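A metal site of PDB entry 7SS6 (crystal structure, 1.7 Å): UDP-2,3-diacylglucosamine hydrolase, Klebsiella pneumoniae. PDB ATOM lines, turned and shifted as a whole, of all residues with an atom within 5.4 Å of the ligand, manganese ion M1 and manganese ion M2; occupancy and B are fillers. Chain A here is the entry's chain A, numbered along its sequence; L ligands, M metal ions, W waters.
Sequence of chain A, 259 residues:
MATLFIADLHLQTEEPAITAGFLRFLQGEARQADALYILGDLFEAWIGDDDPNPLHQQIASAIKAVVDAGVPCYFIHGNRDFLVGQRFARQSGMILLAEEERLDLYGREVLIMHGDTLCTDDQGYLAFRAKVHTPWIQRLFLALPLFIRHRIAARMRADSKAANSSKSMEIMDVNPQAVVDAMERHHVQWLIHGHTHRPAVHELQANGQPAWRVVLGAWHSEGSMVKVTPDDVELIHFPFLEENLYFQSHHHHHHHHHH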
ATOM      1  N   ASP A   8       4.059 -13.677 -16.463  1.00  0.00           N
ATOM      2  CA  ASP A   8       5.216 -13.945 -17.290  1.00  0.00           C
ATOM      3  C   ASP A   8       4.843 -14.263 -18.732  1.00  0.00           C
ATOM      4  O   ASP A   8       5.385 -15.179 -19.353  1.00  0.00           O
ATOM      5  CB  ASP A   8       6.036 -15.071 -16.663  1.00  0.00           C
ATOM      6  CG  ASP A   8       6.578 -14.666 -15.305  1.00  0.00           C
ATOM      7  OD1 ASP A   8       7.357 -13.704 -15.282  1.00  0.00           O
ATOM      8  OD2 ASP A   8       6.239 -15.287 -14.284  1.00  0.00           O
ATOM      9  N   HIS A  10       5.240 -11.745 -21.013  1.00  0.00           N
ATOM     10  CA  HIS A  10       6.270 -10.937 -21.688  1.00  0.00           C
ATOM     11  C   HIS A  10       5.817 -10.532 -23.092  1.00  0.00           C
ATOM     12  O   HIS A  10       6.547 -10.687 -24.070  1.00  0.00           O
ATOM     13  CB  HIS A  10       7.604 -11.696 -21.743  1.00  0.00           C
ATOM     14  CG  HIS A  10       7.972 -12.352 -20.453  1.00  0.00           C
ATOM     15  ND1 HIS A  10       7.943 -13.713 -20.270  1.00  0.00           N
ATOM     16  CD2 HIS A  10       8.370 -11.821 -19.268  1.00  0.00           C
ATOM     17  CE1 HIS A  10       8.294 -14.005 -19.035  1.00  0.00           C
ATOM     18  NE2 HIS A  10       8.552 -12.869 -18.404  1.00  0.00           N
ATOM     19  N   ASP A  41       4.730  -9.118 -15.123  1.00  0.00           N
ATOM     20  CA  ASP A  41       5.402  -9.432 -16.395  1.00  0.00           C
ATOM     21  C   ASP A  41       4.382  -9.815 -17.460  1.00  0.00           C
ATOM     22  O   ASP A  41       4.582 -10.723 -18.274  1.00  0.00           O
ATOM     23  CB  ASP A  41       6.459 -10.528 -16.214  1.00  0.00           C
ATOM     24  CG  ASP A  41       7.681 -10.056 -15.440  1.00  0.00           C
ATOM     25  OD1 ASP A  41       7.756  -8.868 -15.083  1.00  0.00           O
ATOM     26  OD2 ASP A  41       8.559 -10.889 -15.209  1.00  0.00           O
ATOM     27  N   GLU A  44       6.714  -7.354 -21.853  1.00  0.00           N
ATOM     28  CA  GLU A  44       8.165  -7.506 -21.777  1.00  0.00           C
ATOM     29  C   GLU A  44       8.844  -6.218 -21.351  1.00  0.00           C
ATOM     30  O   GLU A  44       9.955  -6.247 -20.799  1.00  0.00           O
ATOM     31  CB  GLU A  44       8.695  -7.973 -23.141  1.00  0.00           C
ATOM     32  CG  GLU A  44      10.239  -7.970 -23.289  1.00  0.00           C
ATOM     33  CD  GLU A  44      10.979  -8.999 -22.444  1.00  0.00           C
ATOM     34  OE1 GLU A  44      10.362  -9.700 -21.629  1.00  0.00           O
ATOM     35  OE2 GLU A  44      12.224  -9.080 -22.588  1.00  0.00           O
ATOM     36  N   ALA A  45       8.192  -5.079 -21.580  1.00  0.00           N
ATOM     37  CA  ALA A  45       8.739  -3.787 -21.213  1.00  0.00           C
ATOM     38  C   ALA A  45       7.587  -2.823 -20.977  1.00  0.00           C
ATOM     39  O   ALA A  45       6.505  -3.000 -21.531  1.00  0.00           O
ATOM     40  CB  ALA A  45       9.664  -3.251 -22.325  1.00  0.00           C
ATOM     41  N   TRP A  46       7.827  -1.794 -20.157  1.00  0.00           N
ATOM     42  CA  TRP A  46       6.869  -0.706 -20.016  1.00  0.00           C
ATOM     43  C   TRP A  46       7.647   0.552 -19.652  1.00  0.00           C
ATOM     44  O   TRP A  46       8.448   0.537 -18.726  1.00  0.00           O
ATOM     45  CB  TRP A  46       5.838  -0.983 -18.913  1.00  0.00           C
ATOM     46  CG  TRP A  46       4.537  -0.201 -19.051  1.00  0.00           C
ATOM     47  CD1 TRP A  46       4.188   0.959 -18.410  1.00  0.00           C
ATOM     48  CD2 TRP A  46       3.413  -0.564 -19.871  1.00  0.00           C
ATOM     49  NE1 TRP A  46       2.903   1.340 -18.794  1.00  0.00           N
ATOM     50  CE2 TRP A  46       2.422   0.422 -19.692  1.00  0.00           C
ATOM     51  CE3 TRP A  46       3.161  -1.632 -20.744  1.00  0.00           C
ATOM     52  CZ2 TRP A  46       1.172   0.351 -20.338  1.00  0.00           C
ATOM     53  CZ3 TRP A  46       1.915  -1.690 -21.394  1.00  0.00           C
ATOM     54  CH2 TRP A  46       0.948  -0.706 -21.175  1.00  0.00           C
ATOM     55  N   ILE A  47       7.398   1.635 -20.392  1.00  0.00           N
ATOM     56  CA  ILE A  47       8.047   2.914 -20.106  1.00  0.00           C
ATOM     57  C   ILE A  47       7.038   3.990 -19.736  1.00  0.00           C
ATOM     58  O   ILE A  47       7.404   5.156 -19.597  1.00  0.00           O
ATOM     59  CB  ILE A  47       8.947   3.371 -21.279  1.00  0.00           C
ATOM     60  CG1 ILE A  47       8.133   3.564 -22.569  1.00  0.00           C
ATOM     61  CG2 ILE A  47      10.106   2.397 -21.474  1.00  0.00           C
ATOM     62  CD1 ILE A  47       8.942   4.155 -23.713  1.00  0.00           C
ATOM     63  N   GLY A  78       5.048  -6.800 -12.347  1.00  0.00           N
ATOM     64  CA  GLY A  78       6.292  -7.545 -12.443  1.00  0.00           C
ATOM     65  C   GLY A  78       7.475  -6.600 -12.498  1.00  0.00           C
ATOM     66  O   GLY A  78       7.332  -5.380 -12.506  1.00  0.00           O
ATOM     67  N   ASN A  79       8.669  -7.183 -12.556  1.00  0.00           N
ATOM     68  CA  ASN A  79       9.865  -6.377 -12.725  1.00  0.00           C
ATOM     69  C   ASN A  79      10.007  -5.838 -14.145  1.00  0.00           C
ATOM     70  O   ASN A  79      10.710  -4.847 -14.346  1.00  0.00           O
ATOM     71  CB  ASN A  79      11.102  -7.187 -12.354  1.00  0.00           C
ATOM     72  CG  ASN A  79      11.228  -8.441 -13.169  1.00  0.00           C
ATOM     73  OD1 ASN A  79      10.432  -9.374 -13.018  1.00  0.00           O
ATOM     74  ND2 ASN A  79      12.238  -8.501 -14.026  1.00  0.00           N
ATOM     75  N   ARG A  80       9.356  -6.469 -15.137  1.00  0.00           N
ATOM     76  CA  ARG A  80       9.412  -5.922 -16.481  1.00  0.00           C
ATOM     77  C   ARG A  80       8.442  -4.758 -16.658  1.00  0.00           C
ATOM     78  O   ARG A  80       8.726  -3.827 -17.438  1.00  0.00           O
ATOM     79  CB  ARG A  80       9.106  -6.999 -17.534  1.00  0.00           C
ATOM     80  CG  ARG A  80       9.968  -8.255 -17.468  1.00  0.00           C
ATOM     81  CD  ARG A  80      11.458  -7.925 -17.652  1.00  0.00           C
ATOM     82  NE  ARG A  80      11.715  -7.326 -18.955  1.00  0.00           N
ATOM     83  CZ  ARG A  80      12.914  -7.232 -19.505  1.00  0.00           C
ATOM     84  NH1 ARG A  80      13.990  -7.749 -18.924  1.00  0.00           N
ATOM     85  NH2 ARG A  80      13.052  -6.607 -20.670  1.00  0.00           N
ATOM     86  N   PHE A  82       6.749  -2.736 -14.131  1.00  0.00           N
ATOM     87  CA  PHE A  82       6.417  -2.034 -12.898  1.00  0.00           C
ATOM     88  C   PHE A  82       5.908  -0.608 -13.139  1.00  0.00           C
ATOM     89  O   PHE A  82       5.317  -0.019 -12.228  1.00  0.00           O
ATOM     90  CB  PHE A  82       7.634  -1.984 -11.949  1.00  0.00           C
ATOM     91  CG  PHE A  82       8.845  -1.284 -12.506  1.00  0.00           C
ATOM     92  CD1 PHE A  82       9.782  -1.984 -13.266  1.00  0.00           C
ATOM     93  CD2 PHE A  82       9.052   0.074 -12.281  1.00  0.00           C
ATOM     94  CE1 PHE A  82      10.909  -1.339 -13.787  1.00  0.00           C
ATOM     95  CE2 PHE A  82      10.171   0.714 -12.802  1.00  0.00           C
ATOM     96  CZ  PHE A  82      11.090   0.004 -13.562  1.00  0.00           C
ATOM     97  N   LEU A  83       6.064  -0.072 -14.339  1.00  0.00           N
ATOM     98  CA  LEU A  83       5.547   1.270 -14.601  1.00  0.00           C
ATOM     99  C   LEU A  83       4.110   1.279 -15.105  1.00  0.00           C
ATOM    100  O   LEU A  83       3.593   2.366 -15.400  1.00  0.00           O
ATOM    101  CB  LEU A  83       6.445   2.005 -15.616  1.00  0.00           C
ATOM    102  CG  LEU A  83       7.837   2.386 -15.095  1.00  0.00           C
ATOM    103  CD1 LEU A  83       8.623   3.095 -16.173  1.00  0.00           C
ATOM    104  CD2 LEU A  83       7.718   3.277 -13.846  1.00  0.00           C
ATOM    105  N   HIS A 114       4.345 -11.282  -7.481  1.00  0.00           N
ATOM    106  CA  HIS A 114       5.071 -11.609  -8.698  1.00  0.00           C
ATOM    107  C   HIS A 114       6.138 -12.662  -8.410  1.00  0.00           C
ATOM    108  O   HIS A 114       6.334 -13.603  -9.188  1.00  0.00           O
ATOM    109  CB  HIS A 114       5.724 -10.379  -9.323  1.00  0.00           C
ATOM    110  CG  HIS A 114       6.461 -10.686 -10.581  1.00  0.00           C
ATOM    111  ND1 HIS A 114       5.857 -11.280 -11.668  1.00  0.00           N
ATOM    112  CD2 HIS A 114       7.775 -10.551 -10.915  1.00  0.00           C
ATOM    113  CE1 HIS A 114       6.742 -11.462 -12.627  1.00  0.00           C
ATOM    114  NE2 HIS A 114       7.916 -11.029 -12.197  1.00  0.00           N
ATOM    115  N   ASP A 116       9.537 -11.843  -7.490  1.00  0.00           N
ATOM    116  CA  ASP A 116      10.936 -11.398  -7.502  1.00  0.00           C
ATOM    117  C   ASP A 116      11.425 -10.961  -6.127  1.00  0.00           C
ATOM    118  O   ASP A 116      12.626 -11.065  -5.833  1.00  0.00           O
ATOM    119  CB  ASP A 116      11.141 -10.258  -8.508  1.00  0.00           C
ATOM    120  CG  ASP A 116      10.245  -9.059  -8.242  1.00  0.00           C
ATOM    121  OD1 ASP A 116       9.019  -9.226  -8.050  1.00  0.00           O
ATOM    122  OD2 ASP A 116      10.771  -7.926  -8.272  1.00  0.00           O
ATOM    123  N   TYR A 125      20.134  -7.381  -7.670  1.00  0.00           N
ATOM    124  CA  TYR A 125      18.820  -7.130  -8.261  1.00  0.00           C
ATOM    125  C   TYR A 125      17.929  -6.348  -7.301  1.00  0.00           C
ATOM    126  O   TYR A 125      17.294  -5.358  -7.684  1.00  0.00           O
ATOM    127  CB  TYR A 125      18.158  -8.445  -8.659  1.00  0.00           C
ATOM    128  CG  TYR A 125      16.701  -8.206  -8.979  1.00  0.00           C
ATOM    129  CD1 TYR A 125      16.354  -7.468 -10.086  1.00  0.00           C
ATOM    130  CD2 TYR A 125      15.711  -8.649  -8.129  1.00  0.00           C
ATOM    131  CE1 TYR A 125      15.028  -7.213 -10.378  1.00  0.00           C
ATOM    132  CE2 TYR A 125      14.374  -8.396  -8.412  1.00  0.00           C
ATOM    133  CZ  TYR A 125      14.047  -7.673  -9.541  1.00  0.00           C
ATOM    134  OH  TYR A 125      12.741  -7.412  -9.843  1.00  0.00           O
ATOM    135  N   PHE A 128      18.764  -2.581  -7.221  1.00  0.00           N
ATOM    136  CA  PHE A 128      18.206  -1.938  -8.408  1.00  0.00           C
ATOM    137  C   PHE A 128      16.680  -1.854  -8.328  1.00  0.00           C
ATOM    138  O   PHE A 128      16.086  -0.834  -8.680  1.00  0.00           O
ATOM    139  CB  PHE A 128      18.619  -2.717  -9.653  1.00  0.00           C
ATOM    140  CG  PHE A 128      17.849  -2.346 -10.887  1.00  0.00           C
ATOM    141  CD1 PHE A 128      18.097  -1.159 -11.554  1.00  0.00           C
ATOM    142  CD2 PHE A 128      16.852  -3.195 -11.378  1.00  0.00           C
ATOM    143  CE1 PHE A 128      17.376  -0.830 -12.689  1.00  0.00           C
ATOM    144  CE2 PHE A 128      16.129  -2.862 -12.504  1.00  0.00           C
ATOM    145  CZ  PHE A 128      16.390  -1.678 -13.167  1.00  0.00           C
ATOM    146  N   VAL A 132      14.304   1.660  -8.740  1.00  0.00           N
ATOM    147  CA  VAL A 132      13.239   1.944  -9.698  1.00  0.00           C
ATOM    148  C   VAL A 132      11.852   1.912  -9.078  1.00  0.00           C
ATOM    149  O   VAL A 132      10.878   2.238  -9.750  1.00  0.00           O
ATOM    150  CB  VAL A 132      13.252   0.996 -10.915  1.00  0.00           C
ATOM    151  CG1 VAL A 132      14.562   1.136 -11.693  1.00  0.00           C
ATOM    152  CG2 VAL A 132      12.990  -0.463 -10.491  1.00  0.00           C
ATOM    153  N   ILE A 137      12.189   8.719  -8.221  1.00  0.00           N
ATOM    154  CA  ILE A 137      12.884   8.228  -9.396  1.00  0.00           C
ATOM    155  C   ILE A 137      11.893   7.877 -10.502  1.00  0.00           C
ATOM    156  O   ILE A 137      12.099   8.230 -11.664  1.00  0.00           O
ATOM    157  CB  ILE A 137      13.794   7.048  -9.014  1.00  0.00           C
ATOM    158  CG1 ILE A 137      14.880   7.515  -8.048  1.00  0.00           C
ATOM    159  CG2 ILE A 137      14.422   6.417 -10.246  1.00  0.00           C
ATOM    160  CD1 ILE A 137      15.846   6.436  -7.617  1.00  0.00           C
ATOM    161  N   GLN A 138      10.795   7.180 -10.163  1.00  0.00           N
ATOM    162  CA  GLN A 138       9.778   6.892 -11.180  1.00  0.00           C
ATOM    163  C   GLN A 138       9.215   8.171 -11.786  1.00  0.00           C
ATOM    164  O   GLN A 138       9.025   8.252 -13.009  1.00  0.00           O
ATOM    165  CB  GLN A 138       8.641   6.067 -10.581  1.00  0.00           C
ATOM    166  CG  GLN A 138       9.035   4.679 -10.185  1.00  0.00           C
ATOM    167  CD  GLN A 138       7.828   3.833  -9.921  1.00  0.00           C
ATOM    168  OE1 GLN A 138       6.698   4.326  -9.965  1.00  0.00           O
ATOM    169  NE2 GLN A 138       8.043   2.550  -9.653  1.00  0.00           N
ATOM    170  N   PHE A 141      11.720   9.663 -14.261  1.00  0.00           N
ATOM    171  CA  PHE A 141      11.787   8.898 -15.512  1.00  0.00           C
ATOM    172  C   PHE A 141      10.579   9.187 -16.385  1.00  0.00           C
ATOM    173  O   PHE A 141      10.703   9.443 -17.582  1.00  0.00           O
ATOM    174  CB  PHE A 141      11.887   7.397 -15.210  1.00  0.00           C
ATOM    175  CG  PHE A 141      11.918   6.537 -16.451  1.00  0.00           C
ATOM    176  CD1 PHE A 141      13.108   6.311 -17.130  1.00  0.00           C
ATOM    177  CD2 PHE A 141      10.759   5.941 -16.928  1.00  0.00           C
ATOM    178  CE1 PHE A 141      13.132   5.501 -18.260  1.00  0.00           C
ATOM    179  CE2 PHE A 141      10.791   5.156 -18.067  1.00  0.00           C
ATOM    180  CZ  PHE A 141      11.959   4.928 -18.729  1.00  0.00           C
ATOM    181  N   ILE A 152      16.366   4.909 -23.678  1.00  0.00           N
ATOM    182  CA  ILE A 152      16.943   4.392 -22.429  1.00  0.00           C
ATOM    183  C   ILE A 152      16.600   2.912 -22.287  1.00  0.00           C
ATOM    184  O   ILE A 152      17.463   2.065 -22.043  1.00  0.00           O
ATOM    185  CB  ILE A 152      16.443   5.181 -21.212  1.00  0.00           C
ATOM    186  CG1 ILE A 152      17.064   6.585 -21.169  1.00  0.00           C
ATOM    187  CG2 ILE A 152      16.722   4.421 -19.922  1.00  0.00           C
ATOM    188  CD1 ILE A 152      16.394   7.483 -20.147  1.00  0.00           C
ATOM    189  N   ALA A 153      15.315   2.588 -22.491  1.00  0.00           N
ATOM    190  CA  ALA A 153      14.851   1.214 -22.292  1.00  0.00           C
ATOM    191  C   ALA A 153      15.492   0.267 -23.300  1.00  0.00           C
ATOM    192  O   ALA A 153      15.896  -0.844 -22.935  1.00  0.00           O
ATOM    193  CB  ALA A 153      13.332   1.169 -22.389  1.00  0.00           C
ATOM    194  N   ALA A 154      15.588   0.689 -24.567  1.00  0.00           N
ATOM    195  CA  ALA A 154      16.183  -0.181 -25.576  1.00  0.00           C
ATOM    196  C   ALA A 154      17.651  -0.440 -25.279  1.00  0.00           C
ATOM    197  O   ALA A 154      18.137  -1.574 -25.445  1.00  0.00           O
ATOM    198  CB  ALA A 154      16.017   0.426 -26.972  1.00  0.00           C
ATOM    199  N   MET A 156      19.026  -0.355 -22.254  1.00  0.00           N
ATOM    200  CA  MET A 156      19.041  -1.200 -21.062  1.00  0.00           C
ATOM    201  C   MET A 156      18.753  -2.656 -21.411  1.00  0.00           C
ATOM    202  O   MET A 156      19.394  -3.578 -20.877  1.00  0.00           O
ATOM    203  CB  MET A 156      17.999  -0.653 -20.082  1.00  0.00           C
ATOM    204  CG  MET A 156      18.405   0.684 -19.502  1.00  0.00           C
ATOM    205  SD  MET A 156      17.599   1.146 -17.960  1.00  0.00           S
ATOM    206  CE  MET A 156      17.528  -0.416 -17.091  1.00  0.00           C
ATOM    207  N   ARG A 157      17.783  -2.887 -22.294  1.00  0.00           N
ATOM    208  CA  ARG A 157      17.484  -4.246 -22.735  1.00  0.00           C
ATOM    209  C   ARG A 157      18.638  -4.823 -23.548  1.00  0.00           C
ATOM    210  O   ARG A 157      18.999  -6.000 -23.379  1.00  0.00           O
ATOM    211  CB  ARG A 157      16.188  -4.279 -23.533  1.00  0.00           C
ATOM    212  CG  ARG A 157      14.934  -3.985 -22.698  1.00  0.00           C
ATOM    213  CD  ARG A 157      13.667  -4.302 -23.475  1.00  0.00           C
ATOM    214  NE  ARG A 157      13.577  -3.528 -24.711  1.00  0.00           N
ATOM    215  CZ  ARG A 157      13.034  -2.317 -24.796  1.00  0.00           C
ATOM    216  NH1 ARG A 157      12.496  -1.720 -23.752  1.00  0.00           N
ATOM    217  NH2 ARG A 157      13.024  -1.697 -25.976  1.00  0.00           N
ATOM    218  N   SER A 160      21.331  -5.807 -21.074  1.00  0.00           N
ATOM    219  CA  SER A 160      21.049  -6.954 -20.220  1.00  0.00           C
ATOM    220  C   SER A 160      21.121  -8.275 -20.985  1.00  0.00           C
ATOM    221  O   SER A 160      21.405  -9.319 -20.389  1.00  0.00           O
ATOM    222  CB  SER A 160      19.684  -6.806 -19.563  1.00  0.00           C
ATOM    223  OG  SER A 160      19.731  -5.882 -18.488  1.00  0.00           O
ATOM    224  N   ILE A 171      17.608 -17.225 -14.367  1.00  0.00           N
ATOM    225  CA  ILE A 171      16.940 -16.429 -13.343  1.00  0.00           C
ATOM    226  C   ILE A 171      17.198 -17.034 -11.970  1.00  0.00           C
ATOM    227  O   ILE A 171      16.981 -18.235 -11.750  1.00  0.00           O
ATOM    228  CB  ILE A 171      15.435 -16.322 -13.639  1.00  0.00           C
ATOM    229  CG1 ILE A 171      15.207 -15.962 -15.121  1.00  0.00           C
ATOM    230  CG2 ILE A 171      14.727 -15.380 -12.658  1.00  0.00           C
ATOM    231  CD1 ILE A 171      13.746 -15.893 -15.523  1.00  0.00           C
ATOM    232  N   HIS A 195       7.646 -15.081 -11.980  1.00  0.00           N
ATOM    233  CA  HIS A 195       9.015 -14.566 -12.019  1.00  0.00           C
ATOM    234  C   HIS A 195      10.105 -15.603 -12.273  1.00  0.00           C
ATOM    235  O   HIS A 195      10.992 -15.356 -13.108  1.00  0.00           O
ATOM    236  CB  HIS A 195       9.358 -13.806 -10.748  1.00  0.00           C
ATOM    237  CG  HIS A 195      10.705 -13.138 -10.817  1.00  0.00           C
ATOM    238  ND1 HIS A 195      10.975 -12.087 -11.665  1.00  0.00           N
ATOM    239  CD2 HIS A 195      11.867 -13.390 -10.163  1.00  0.00           C
ATOM    240  CE1 HIS A 195      12.239 -11.710 -11.525  1.00  0.00           C
ATOM    241  NE2 HIS A 195      12.798 -12.492 -10.613  1.00  0.00           N
ATOM    242  N   THR A 196      10.091 -16.733 -11.569  1.00  0.00           N
ATOM    243  CA  THR A 196      11.212 -17.662 -11.694  1.00  0.00           C
ATOM    244  C   THR A 196      11.137 -18.522 -12.941  1.00  0.00           C
ATOM    245  O   THR A 196      12.110 -19.203 -13.271  1.00  0.00           O
ATOM    246  CB  THR A 196      11.311 -18.550 -10.461  1.00  0.00           C
ATOM    247  OG1 THR A 196      10.115 -19.357 -10.359  1.00  0.00           O
ATOM    248  CG2 THR A 196      11.468 -17.693  -9.193  1.00  0.00           C
ATOM    249  N   HIS A 197       9.993 -18.536 -13.640  1.00  0.00           N
ATOM    250  CA  HIS A 197       9.817 -19.264 -14.893  1.00  0.00           C
ATOM    251  C   HIS A 197      10.045 -20.764 -14.715  1.00  0.00           C
ATOM    252  O   HIS A 197      10.495 -21.448 -15.643  1.00  0.00           O
ATOM    253  CB  HIS A 197      10.734 -18.717 -15.977  1.00  0.00           C
ATOM    254  CG  HIS A 197      10.461 -17.278 -16.342  1.00  0.00           C
ATOM    255  ND1 HIS A 197      11.112 -16.654 -17.384  1.00  0.00           N
ATOM    256  CD2 HIS A 197       9.610 -16.370 -15.821  1.00  0.00           C
ATOM    257  CE1 HIS A 197      10.664 -15.408 -17.483  1.00  0.00           C
ATOM    258  NE2 HIS A 197       9.774 -15.198 -16.538  1.00  0.00           N
HETATM  259  C1  LIG L   1      12.447  -3.692 -17.581  1.00  0.00           C
HETATM  260  C2  LIG L   1      14.487  -4.915 -17.232  1.00  0.00           C
HETATM  261  C3  LIG L   1      14.411  -3.304 -19.006  1.00  0.00           C
HETATM  262  C4  LIG L   1      15.086  -6.880 -15.669  1.00  0.00           C
HETATM  263  C5  LIG L   1      15.788  -8.822 -14.213  1.00  0.00           C
HETATM  264  C6  LIG L   1      14.786 -11.172 -14.103  1.00  0.00           C
HETATM  265  C7  LIG L   1      12.538 -12.069 -14.788  1.00  0.00           C
HETATM  266  C8  LIG L   1      12.656   2.983 -15.054  1.00  0.00           C
HETATM  267  C9  LIG L   1      13.577   2.604 -16.006  1.00  0.00           C
HETATM  268  C10 LIG L   1      13.840   1.563 -18.277  1.00  0.00           C
HETATM  269  C11 LIG L   1      13.847   0.099 -18.691  1.00  0.00           C
HETATM  270  C12 LIG L   1      11.773  -0.222 -17.527  1.00  0.00           C
HETATM  271  C13 LIG L   1      11.778   1.203 -17.013  1.00  0.00           C
HETATM  272  C14 LIG L   1      13.104  -3.060 -18.637  1.00  0.00           C
HETATM  273  C15 LIG L   1      13.147  -4.654 -16.867  1.00  0.00           C
HETATM  274  C16 LIG L   1      15.124  -4.269 -18.288  1.00  0.00           C
HETATM  275  C17 LIG L   1      16.555  -4.780 -18.439  1.00  0.00           C
HETATM  276  C18 LIG L   1      16.744  -5.741 -17.285  1.00  0.00           C
HETATM  277  C19 LIG L   1      15.103  -9.964 -15.021  1.00  0.00           C
HETATM  278  C20 LIG L   1      14.050 -12.286 -14.880  1.00  0.00           C
HETATM  279  C21 LIG L   1      14.865   3.117 -16.055  1.00  0.00           C
HETATM  280  C22 LIG L   1      15.232   4.032 -15.094  1.00  0.00           C
HETATM  281  C23 LIG L   1      14.348   4.428 -14.107  1.00  0.00           C
HETATM  282  C24 LIG L   1      13.056   3.881 -14.089  1.00  0.00           C
HETATM  283  C25 LIG L   1      16.654   4.593 -15.152  1.00  0.00           C
HETATM  284  F1  LIG L   1      17.510   3.542 -15.112  1.00  0.00           F
HETATM  285  F2  LIG L   1      16.840   5.402 -14.079  1.00  0.00           F
HETATM  286  F3  LIG L   1      16.841   5.273 -16.296  1.00  0.00           F
HETATM  287  N1  LIG L   1      13.174   1.652 -16.993  1.00  0.00           N
HETATM  288  N2  LIG L   1      12.450  -0.330 -18.810  1.00  0.00           N
HETATM  289  N3  LIG L   1      15.439  -5.891 -16.659  1.00  0.00           N
HETATM  290  N4  LIG L   1      16.133  -7.801 -15.209  1.00  0.00           N
HETATM  291  N5  LIG L   1      11.634 -13.190 -14.581  1.00  0.00           N
HETATM  292  O1  LIG L   1      12.739  -1.805 -20.936  1.00  0.00           O
HETATM  293  O2  LIG L   1      10.784  -2.111 -19.556  1.00  0.00           O
HETATM  294  O3  LIG L   1      13.991  -6.914 -15.232  1.00  0.00           O
HETATM  295  O4  LIG L   1      12.046 -10.984 -14.872  1.00  0.00           O
HETATM  296  O5  LIG L   1      10.267 -12.865 -14.521  1.00  0.00           O
HETATM  297  S1  LIG L   1      12.226  -1.817 -19.579  1.00  0.00           S
HETATM  298 CL1  LIG L   1      11.903   4.361 -12.849  1.00  0.00          CL
HETATM  299 MN    MN M   1       9.051 -13.037 -16.216  1.00  0.00          MN
HETATM  300 MN    MN M   2       9.791 -11.196 -13.454  1.00  0.00          MN
HETATM  301  O   HOH W   1      13.546 -10.938 -17.865  1.00  0.00           O
HETATM  302  O   HOH W   2      10.975 -11.853 -17.107  1.00  0.00           O
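A nitrogen (N5) of the ligand lies within hydrogen-bond range of the backbone carbonyl oxygen (O) of His 195, at 2.7 Å.
NH1 of Arg 157 lies within hydrogen-bond range of O1 of the ligand (2.8 Å).
N of Trp 46 sits at hydrogen-bond distance from O2 of the ligand (3.0 Å).
The backbone NH of His 195 is in hydrogen-bond range of the side-chain carboxylate of Asp 8 (2.7 Å).
The side-chain carboxylate (OD1) of Asp 41 lies within hydrogen-bond range of the backbone NH (N) of Arg 80, 2.9 Å away.
The backbone carbonyl oxygen (O) of Met 156 lies within hydrogen-bond range of the side-chain hydroxyl (OG) of Ser 160.
The side-chain carboxylate (OE2) of Glu 44 lies within salt-bridge range of the guanidinium group (NH2) of Arg 80 (3.2 Å).
The side-chain amide nitrogen of Gln 138 sits at hydrogen-bond distance from the backbone carbonyl oxygen of Val 132 (2.9 Å).
N3 of the ligand lies close to NH1 of Arg 80 (3.3 Å).
The side-chain sulfur of Met 156 sits close to a fluorine (F1) of the ligand, 3.7 Å away.
Ala 45 touches the ligand.
Phe 82 touches the ligand.
CD1 of Leu 83 touches C13 of the ligand, at 3.8 Å.
Val 132 touches the ligand (O to CL1, 3.9 Å).
Gln 138 touches the ligand (CA to CL1, 3.7 Å).
Phe 141 touches the ligand.
Ile 152 touches the ligand.
Ala 153 touches the ligand (CB to O1, 3.4 Å).
Ser 160 touches the ligand.
Ile 171 touches the ligand.
Hydrophobic or aromatic side chains that line the ligand: Ala 45, Phe 82, Leu 83, Val 132, Phe 141, Ile 152, Ala 153, Met 156, Ile 171, His 195 and His 197.
20 residues have an atom within 4 Å of the ligand: Asp 8, Asp 41, Ala 45, Trp 46, Asn 79, Arg 80, Phe 82, Leu 83, His 114, Val 132, Gln 138, Phe 141, Ile 152, Ala 153, Met 156, Arg 157, Ser 160, Ile 171, His 195 and His 197.
The nearest printed residue that does not touch the ligand is Ile 137 (4.1 Å).
Of the 30 residues printed, 4 come within 4 Å of manganese ion M1.
The nearest printed residue that does not touch manganese ion M1 is His 195 (4.3 Å).
Five residues have an atom within 4 Å of manganese ion M2: Asp 8, Asp 41, Asn 79, His 114 and His 195.
The nearest printed residue that does not touch manganese ion M2 is Arg 80 (5.0 Å).
OD1 of Asp 8 binds manganese ion M1, 2.0 Å away.
Manganese ion M1 is bound by O5 of the ligand (2.1 Å).
Manganese ion M1 is bound by NE2 of His 10.
A ring nitrogen (NE2) of His 197 binds manganese ion M1, at 2.3 Å.
The side-chain carboxylate (OD2) of Asp 41 binds manganese ion M1 (2.4 Å).
Manganese ion M1 is bound by water W2, at 2.4 Å.
Manganese ion M1 has six donor atoms within binding distance.
The side-chain amide oxygen (OD1) of Asn 79 is bound to manganese ion M2 (2.0 Å).
O5 of the ligand is bound to manganese ion M2 (2.0 Å).
OD2 of Asp 41 binds manganese ion M2.
Manganese ion M2 is bound by NE2 of His 114.
Manganese ion M2 is bound by ND1 of His 195, at 2.3 Å.
An oxygen (O4) of the ligand is bound to manganese ion M2.
Manganese ion M2 has six donor atoms within binding distance.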
